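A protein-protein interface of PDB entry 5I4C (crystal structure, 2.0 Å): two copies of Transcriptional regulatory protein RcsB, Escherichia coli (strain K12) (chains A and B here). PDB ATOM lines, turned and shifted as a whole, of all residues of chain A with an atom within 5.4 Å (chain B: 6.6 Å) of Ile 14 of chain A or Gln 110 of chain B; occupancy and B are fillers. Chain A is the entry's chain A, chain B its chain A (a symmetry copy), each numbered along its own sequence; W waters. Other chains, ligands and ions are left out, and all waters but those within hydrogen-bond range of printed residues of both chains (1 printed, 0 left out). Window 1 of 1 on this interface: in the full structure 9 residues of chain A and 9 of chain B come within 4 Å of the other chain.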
ATOM      1  N   HIS A  12     -30.872 -20.458   9.900  1.00  0.00           N
ATOM      2  CA  HIS A  12     -30.038 -20.222  11.067  1.00  0.00           C
ATOM      3  C   HIS A  12     -28.614 -19.956  10.608  1.00  0.00           C
ATOM      4  O   HIS A  12     -27.992 -20.858  10.062  1.00  0.00           O
ATOM      5  CB  HIS A  12     -30.087 -21.432  11.996  1.00  0.00           C
ATOM      6  CG  HIS A  12     -31.301 -21.476  12.850  1.00  0.00           C
ATOM      7  ND1 HIS A  12     -32.310 -22.378  12.638  1.00  0.00           N
ATOM      8  CD2 HIS A  12     -31.709 -20.684  13.849  1.00  0.00           C
ATOM      9  CE1 HIS A  12     -33.256 -22.189  13.534  1.00  0.00           C
ATOM     10  NE2 HIS A  12     -32.921 -21.146  14.266  1.00  0.00           N
ATOM     11  N   PRO A  13     -28.107 -18.720  10.788  1.00  0.00           N
ATOM     12  CA  PRO A  13     -26.785 -18.395  10.282  1.00  0.00           C
ATOM     13  C   PRO A  13     -25.719 -19.325  10.848  1.00  0.00           C
ATOM     14  O   PRO A  13     -24.833 -19.707  10.136  1.00  0.00           O
ATOM     15  CB  PRO A  13     -26.579 -16.956  10.734  1.00  0.00           C
ATOM     16  CG  PRO A  13     -27.941 -16.412  10.699  1.00  0.00           C
ATOM     17  CD  PRO A  13     -28.842 -17.514  11.166  1.00  0.00           C
ATOM     18  N   ILE A  14     -25.817 -19.741  12.115  1.00  0.00           N
ATOM     19  CA  ILE A  14     -24.792 -20.657  12.631  1.00  0.00           C
ATOM     20  C   ILE A  14     -24.788 -22.030  11.963  1.00  0.00           C
ATOM     21  O   ILE A  14     -23.773 -22.674  11.991  1.00  0.00           O
ATOM     22  CB  ILE A  14     -24.817 -20.779  14.193  1.00  0.00           C
ATOM     23  CG1 ILE A  14     -23.391 -21.059  14.738  1.00  0.00           C
ATOM     24  CG2 ILE A  14     -25.808 -21.781  14.615  1.00  0.00           C
ATOM     25  CD1 ILE A  14     -23.241 -20.639  16.165  1.00  0.00           C
ATOM     26  N   VAL A  15     -25.923 -22.503  11.465  1.00  0.00           N
ATOM     27  CA  VAL A  15     -25.957 -23.742  10.706  1.00  0.00           C
ATOM     28  C   VAL A  15     -25.160 -23.585   9.413  1.00  0.00           C
ATOM     29  O   VAL A  15     -24.318 -24.448   9.050  1.00  0.00           O
ATOM     30  CB  VAL A  15     -27.419 -24.206  10.430  1.00  0.00           C
ATOM     31  CG1 VAL A  15     -27.453 -25.419   9.518  1.00  0.00           C
ATOM     32  CG2 VAL A  15     -28.180 -24.513  11.723  1.00  0.00           C
ATOM     33  N   LEU A  16     -25.399 -22.477   8.733  1.00  0.00           N
ATOM     34  CA  LEU A  16     -24.664 -22.191   7.502  1.00  0.00           C
ATOM     35  C   LEU A  16     -23.145 -22.064   7.745  1.00  0.00           C
ATOM     36  O   LEU A  16     -22.359 -22.585   6.968  1.00  0.00           O
ATOM     37  CB  LEU A  16     -25.228 -20.973   6.824  1.00  0.00           C
ATOM     38  CG  LEU A  16     -26.698 -21.086   6.386  1.00  0.00           C
ATOM     39  CD1 LEU A  16     -27.144 -19.737   5.841  1.00  0.00           C
ATOM     40  CD2 LEU A  16     -26.909 -22.213   5.422  1.00  0.00           C
ATOM     41  N   PHE A  17     -22.756 -21.390   8.815  1.00  0.00           N
ATOM     42  CA  PHE A  17     -21.349 -21.268   9.210  1.00  0.00           C
ATOM     43  C   PHE A  17     -20.701 -22.634   9.392  1.00  0.00           C
ATOM     44  O   PHE A  17     -19.614 -22.881   8.841  1.00  0.00           O
ATOM     45  CB  PHE A  17     -21.272 -20.474  10.524  1.00  0.00           C
ATOM     46  CG  PHE A  17     -19.892 -20.271  11.032  1.00  0.00           C
ATOM     47  CD1 PHE A  17     -19.074 -19.326  10.478  1.00  0.00           C
ATOM     48  CD2 PHE A  17     -19.399 -21.044  12.021  1.00  0.00           C
ATOM     49  CE1 PHE A  17     -17.778 -19.148  10.982  1.00  0.00           C
ATOM     50  CE2 PHE A  17     -18.111 -20.935  12.495  1.00  0.00           C
ATOM     51  CZ  PHE A  17     -17.297 -19.947  12.001  1.00  0.00           C
ATOM     52  N   GLY A  18     -21.333 -23.514  10.187  1.00  0.00           N
ATOM     53  CA  GLY A  18     -20.767 -24.861  10.493  1.00  0.00           C
ATOM     54  C   GLY A  18     -20.593 -25.683   9.230  1.00  0.00           C
ATOM     55  O   GLY A  18     -19.549 -26.271   8.996  1.00  0.00           O
ATOM     56  N   ILE A  19     -21.639 -25.676   8.397  1.00  0.00           N
ATOM     57  CA  ILE A  19     -21.606 -26.356   7.130  1.00  0.00           C
ATOM     58  C   ILE A  19     -20.482 -25.803   6.231  1.00  0.00           C
ATOM     59  O   ILE A  19     -19.695 -26.566   5.688  1.00  0.00           O
ATOM     60  CB  ILE A  19     -22.985 -26.326   6.438  1.00  0.00           C
ATOM     61  CG1 ILE A  19     -23.952 -27.163   7.289  1.00  0.00           C
ATOM     62  CG2 ILE A  19     -22.843 -26.917   5.036  1.00  0.00           C
ATOM     63  CD1 ILE A  19     -25.392 -27.212   6.809  1.00  0.00           C
ATOM     64  N   ILE B  14     -24.380 -28.627  16.508  1.00  0.00           N
ATOM     65  CA  ILE B  14     -23.835 -27.694  15.514  1.00  0.00           C
ATOM     66  C   ILE B  14     -23.489 -26.317  16.075  1.00  0.00           C
ATOM     67  O   ILE B  14     -22.674 -25.652  15.490  1.00  0.00           O
ATOM     68  CB  ILE B  14     -24.729 -27.582  14.231  1.00  0.00           C
ATOM     69  CG1 ILE B  14     -23.855 -27.276  12.987  1.00  0.00           C
ATOM     70  CG2 ILE B  14     -25.808 -26.603  14.440  1.00  0.00           C
ATOM     71  CD1 ILE B  14     -24.516 -27.702  11.715  1.00  0.00           C
ATOM     72  N   VAL B  15     -24.163 -25.864  17.124  1.00  0.00           N
ATOM     73  CA  VAL B  15     -23.794 -24.622  17.780  1.00  0.00           C
ATOM     74  C   VAL B  15     -22.409 -24.754  18.410  1.00  0.00           C
ATOM     75  O   VAL B  15     -21.525 -23.871  18.247  1.00  0.00           O
ATOM     76  CB  VAL B  15     -24.863 -24.186  18.827  1.00  0.00           C
ATOM     77  CG1 VAL B  15     -24.408 -22.968  19.611  1.00  0.00           C
ATOM     78  CG2 VAL B  15     -26.221 -23.903  18.180  1.00  0.00           C
ATOM     79  N   LEU B  16     -22.205 -25.862  19.100  1.00  0.00           N
ATOM     80  CA  LEU B  16     -20.903 -26.126  19.711  1.00  0.00           C
ATOM     81  C   LEU B  16     -19.775 -26.223  18.662  1.00  0.00           C
ATOM     82  O   LEU B  16     -18.701 -25.681  18.872  1.00  0.00           O
ATOM     83  CB  LEU B  16     -20.969 -27.350  20.581  1.00  0.00           C
ATOM     84  CG  LEU B  16     -21.948 -27.265  21.764  1.00  0.00           C
ATOM     85  CD1 LEU B  16     -21.987 -28.619  22.457  1.00  0.00           C
ATOM     86  CD2 LEU B  16     -21.608 -26.137  22.690  1.00  0.00           C
ATOM     87  N   GLY B  18     -19.661 -24.752  15.634  1.00  0.00           N
ATOM     88  CA  GLY B  18     -19.389 -23.395  15.073  1.00  0.00           C
ATOM     89  C   GLY B  18     -18.557 -22.561  16.030  1.00  0.00           C
ATOM     90  O   GLY B  18     -17.573 -21.951  15.646  1.00  0.00           O
ATOM     91  N   ILE B  19     -18.963 -22.585  17.304  1.00  0.00           N
ATOM     92  CA  ILE B  19     -18.242 -21.897  18.342  1.00  0.00           C
ATOM     93  C   ILE B  19     -16.797 -22.420  18.459  1.00  0.00           C
ATOM     94  O   ILE B  19     -15.857 -21.638  18.476  1.00  0.00           O
ATOM     95  CB  ILE B  19     -19.001 -21.951  19.685  1.00  0.00           C
ATOM     96  CG1 ILE B  19     -20.295 -21.139  19.523  1.00  0.00           C
ATOM     97  CG2 ILE B  19     -18.115 -21.348  20.774  1.00  0.00           C
ATOM     98  CD1 ILE B  19     -21.224 -21.116  20.723  1.00  0.00           C
ATOM     99  N   THR B  87     -28.193 -16.152  23.378  1.00  0.00           N
ATOM    100  CA  THR B  87     -29.601 -15.964  23.357  1.00  0.00           C
ATOM    101  C   THR B  87     -30.169 -16.078  21.946  1.00  0.00           C
ATOM    102  O   THR B  87     -29.568 -15.676  20.956  1.00  0.00           O
ATOM    103  CB  THR B  87     -29.990 -14.661  24.083  1.00  0.00           C
ATOM    104  OG1 THR B  87     -31.390 -14.689  24.223  1.00  0.00           O
ATOM    105  CG2 THR B  87     -29.560 -13.455  23.361  1.00  0.00           C
ATOM    106  N   MET B  88     -31.339 -16.653  21.853  1.00  0.00           N
ATOM    107  CA  MET B  88     -31.908 -16.888  20.520  1.00  0.00           C
ATOM    108  C   MET B  88     -32.539 -15.612  20.021  1.00  0.00           C
ATOM    109  O   MET B  88     -32.845 -15.511  18.854  1.00  0.00           O
ATOM    110  CB  MET B  88     -32.882 -18.082  20.471  1.00  0.00           C
ATOM    111  CG  MET B  88     -32.658 -19.054  19.260  1.00  0.00           C
ATOM    112  SD  MET B  88     -31.537 -18.586  17.861  1.00  0.00           S
ATOM    113  CE  MET B  88     -32.700 -18.063  16.574  1.00  0.00           C
ATOM    114  N   VAL B 107     -24.732 -12.634  24.072  1.00  0.00           N
ATOM    115  CA  VAL B 107     -24.421 -12.702  22.623  1.00  0.00           C
ATOM    116  C   VAL B 107     -25.561 -13.373  21.923  1.00  0.00           C
ATOM    117  O   VAL B 107     -26.005 -14.417  22.389  1.00  0.00           O
ATOM    118  CB  VAL B 107     -23.153 -13.562  22.433  1.00  0.00           C
ATOM    119  CG1 VAL B 107     -22.908 -13.960  20.955  1.00  0.00           C
ATOM    120  CG2 VAL B 107     -21.973 -12.768  22.983  1.00  0.00           C
ATOM    121  N   LEU B 108     -25.974 -12.851  20.784  1.00  0.00           N
ATOM    122  CA  LEU B 108     -26.977 -13.538  19.998  1.00  0.00           C
ATOM    123  C   LEU B 108     -26.354 -14.796  19.453  1.00  0.00           C
ATOM    124  O   LEU B 108     -25.332 -14.751  18.781  1.00  0.00           O
ATOM    125  CB  LEU B 108     -27.516 -12.699  18.869  1.00  0.00           C
ATOM    126  CG  LEU B 108     -28.130 -11.397  19.283  1.00  0.00           C
ATOM    127  CD1 LEU B 108     -28.570 -10.584  18.048  1.00  0.00           C
ATOM    128  CD2 LEU B 108     -29.297 -11.730  20.180  1.00  0.00           C
ATOM    129  N   LYS B 109     -26.979 -15.924  19.772  1.00  0.00           N
ATOM    130  CA  LYS B 109     -26.414 -17.221  19.449  1.00  0.00           C
ATOM    131  C   LYS B 109     -26.072 -17.312  17.969  1.00  0.00           C
ATOM    132  O   LYS B 109     -25.017 -17.821  17.570  1.00  0.00           O
ATOM    133  CB  LYS B 109     -27.436 -18.311  19.821  1.00  0.00           C
ATOM    134  CG  LYS B 109     -26.873 -19.705  19.693  1.00  0.00           C
ATOM    135  CD  LYS B 109     -27.922 -20.812  19.715  1.00  0.00           C
ATOM    136  CE  LYS B 109     -28.447 -20.946  21.076  1.00  0.00           C
ATOM    137  NZ  LYS B 109     -29.048 -22.265  21.280  1.00  0.00           N
ATOM    138  N   GLN B 110     -26.965 -16.881  17.116  1.00  0.00           N
ATOM    139  CA  GLN B 110     -26.687 -17.067  15.676  1.00  0.00           C
ATOM    140  C   GLN B 110     -25.475 -16.272  15.163  1.00  0.00           C
ATOM    141  O   GLN B 110     -24.964 -16.567  14.122  1.00  0.00           O
ATOM    142  CB  GLN B 110     -27.914 -16.793  14.848  1.00  0.00           C
ATOM    143  CG  GLN B 110     -29.069 -17.746  15.179  1.00  0.00           C
ATOM    144  CD  GLN B 110     -28.722 -19.202  14.883  1.00  0.00           C
ATOM    145  OE1 GLN B 110     -28.134 -19.494  13.844  1.00  0.00           O
ATOM    146  NE2 GLN B 110     -29.094 -20.133  15.829  1.00  0.00           N
ATOM    147  N   GLY B 111     -25.069 -15.249  15.890  1.00  0.00           N
ATOM    148  CA  GLY B 111     -23.900 -14.450  15.552  1.00  0.00           C
ATOM    149  C   GLY B 111     -22.695 -14.812  16.404  1.00  0.00           C
ATOM    150  O   GLY B 111     -21.693 -14.164  16.316  1.00  0.00           O
ATOM    151  N   ALA B 112     -22.769 -15.886  17.188  1.00  0.00           N
ATOM    152  CA  ALA B 112     -21.654 -16.221  18.070  1.00  0.00           C
ATOM    153  C   ALA B 112     -20.256 -16.351  17.447  1.00  0.00           C
ATOM    154  O   ALA B 112     -19.288 -15.885  18.039  1.00  0.00           O
ATOM    155  CB  ALA B 112     -22.014 -17.459  18.905  1.00  0.00           C
ATOM    156  N   PRO B 113     -20.133 -16.923  16.227  1.00  0.00           N
ATOM    157  CA  PRO B 113     -18.772 -17.064  15.728  1.00  0.00           C
ATOM    158  C   PRO B 113     -18.053 -15.771  15.511  1.00  0.00           C
ATOM    159  O   PRO B 113     -16.870 -15.741  15.789  1.00  0.00           O
ATOM    160  CB  PRO B 113     -18.936 -17.780  14.375  1.00  0.00           C
ATOM    161  CG  PRO B 113     -20.251 -18.513  14.490  1.00  0.00           C
ATOM    162  CD  PRO B 113     -21.117 -17.662  15.399  1.00  0.00           C
ATOM    163  N   THR B 114     -18.736 -14.745  15.013  1.00  0.00           N
ATOM    164  CA  THR B 114     -18.233 -13.365  14.953  1.00  0.00           C
ATOM    165  C   THR B 114     -18.227 -12.591  16.279  1.00  0.00           C
ATOM    166  O   THR B 114     -17.285 -11.857  16.621  1.00  0.00           O
ATOM    167  CB  THR B 114     -19.139 -12.526  14.044  1.00  0.00           C
ATOM    168  OG1 THR B 114     -19.464 -13.290  12.896  1.00  0.00           O
ATOM    169  CG2 THR B 114     -18.431 -11.248  13.645  1.00  0.00           C
ATOM    170  N   ASP B 115     -19.294 -12.727  17.040  1.00  0.00           N
ATOM    171  CA  ASP B 115     -19.473 -11.844  18.195  1.00  0.00           C
ATOM    172  C   ASP B 115     -18.747 -12.333  19.389  1.00  0.00           C
ATOM    173  O   ASP B 115     -18.363 -11.498  20.211  1.00  0.00           O
ATOM    174  CB  ASP B 115     -20.947 -11.656  18.542  1.00  0.00           C
ATOM    175  CG  ASP B 115     -21.735 -10.957  17.437  1.00  0.00           C
ATOM    176  OD1 ASP B 115     -21.088 -10.291  16.584  1.00  0.00           O
ATOM    177  OD2 ASP B 115     -22.995 -11.100  17.386  1.00  0.00           O
HETATM  178  O   HOH W   1     -21.720 -24.147  13.283  1.00  0.00           O
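N of Lys 109 of chain B lies within hydrogen-bond range of O of Thr 87 of chain B, at 2.9 Å. The side-chain sulfur (SD) of Met 88 of chain B sits at hydrogen-bond distance from the side-chain amide nitrogen (NE2) of Gln 110 of chain B (3.5 Å).
Met 88 of chain B touches His 12 of chain A (CE to NE2, 3.9 Å). Gln 110 of chain B touches His 12 of chain A. Ile 14 of chain A touches Lys 109 of chain B. Ile 14 of chain A touches Pro 113 of chain B. Phe 17 of chain A touches Gly 18 of chain B (CE2 to O, 3.4 Å). CZ of Phe 17 of chain A touches CB of Pro 113 of chain B (3.6 Å).
Of the 8 printed residues of chain A, 4 touch a printed residue of chain B. Hydrophobic or aromatic side chains of chain A that line the printed part of chain B: His 12, Pro 13, Ile 14 and Phe 17. Along chain A the printed residues that touch a printed residue of chain B span positions 12 to 17. Among the printed residues, 8 pairs touch across the chains. Among the printed residues, no Asp or Glu carboxylate lies within 4 Å of a Lys or Arg side-chain nitrogen of the other chain.
Water W1 lies within hydrogen-bond range of O of Ile 14 of chain B, O of Ile 14 of chain A, N of Gly 18 of chain B and N of Gly 18 of chain A.
The backbone NH (N) of Ile 14 of chain A sits at hydrogen-bond distance from the side-chain amide oxygen (OE1) of Gln 110 of chain B, at 2.9 Å. N of Pro 13 of chain A lies close to OE1 of Gln 110 of chain B.
Of chain B, only Lys 109, Gln 110 and Pro 113 come within 4 Å of Ile 14 of chain A. Gln 110 of chain B touches just these residues of chain A: His 12 (3.3 Å), Pro 13 (3.2 Å) and Ile 14 (2.9 Å). Of the printed residues of chain B, Pro 13 of chain A touches Gln 110. Of the printed residues of chain B, His 12 of chain A touches Met 88 (3.9 Å) and Gln 110 (3.3 Å). Of the printed residues of chain B, Phe 17 of chain A touches Gly 18 (3.4 Å) and Pro 113 (3.6 Å). Thr 87 of chain B touches none of the printed residues of chain A. The nearest residue of chain B that does not touch Ile 14 of chain A is Val 15 of chain B (4.2 Å). The nearest residue of chain A that does not touch Gln 110 of chain B is Val 15 of chain A (4.4 Å). The nearest printed residue of chain B that does not touch Pro 13 of chain A is Gly 111 of chain B (5.6 Å).
5 positions are printed for both chains.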
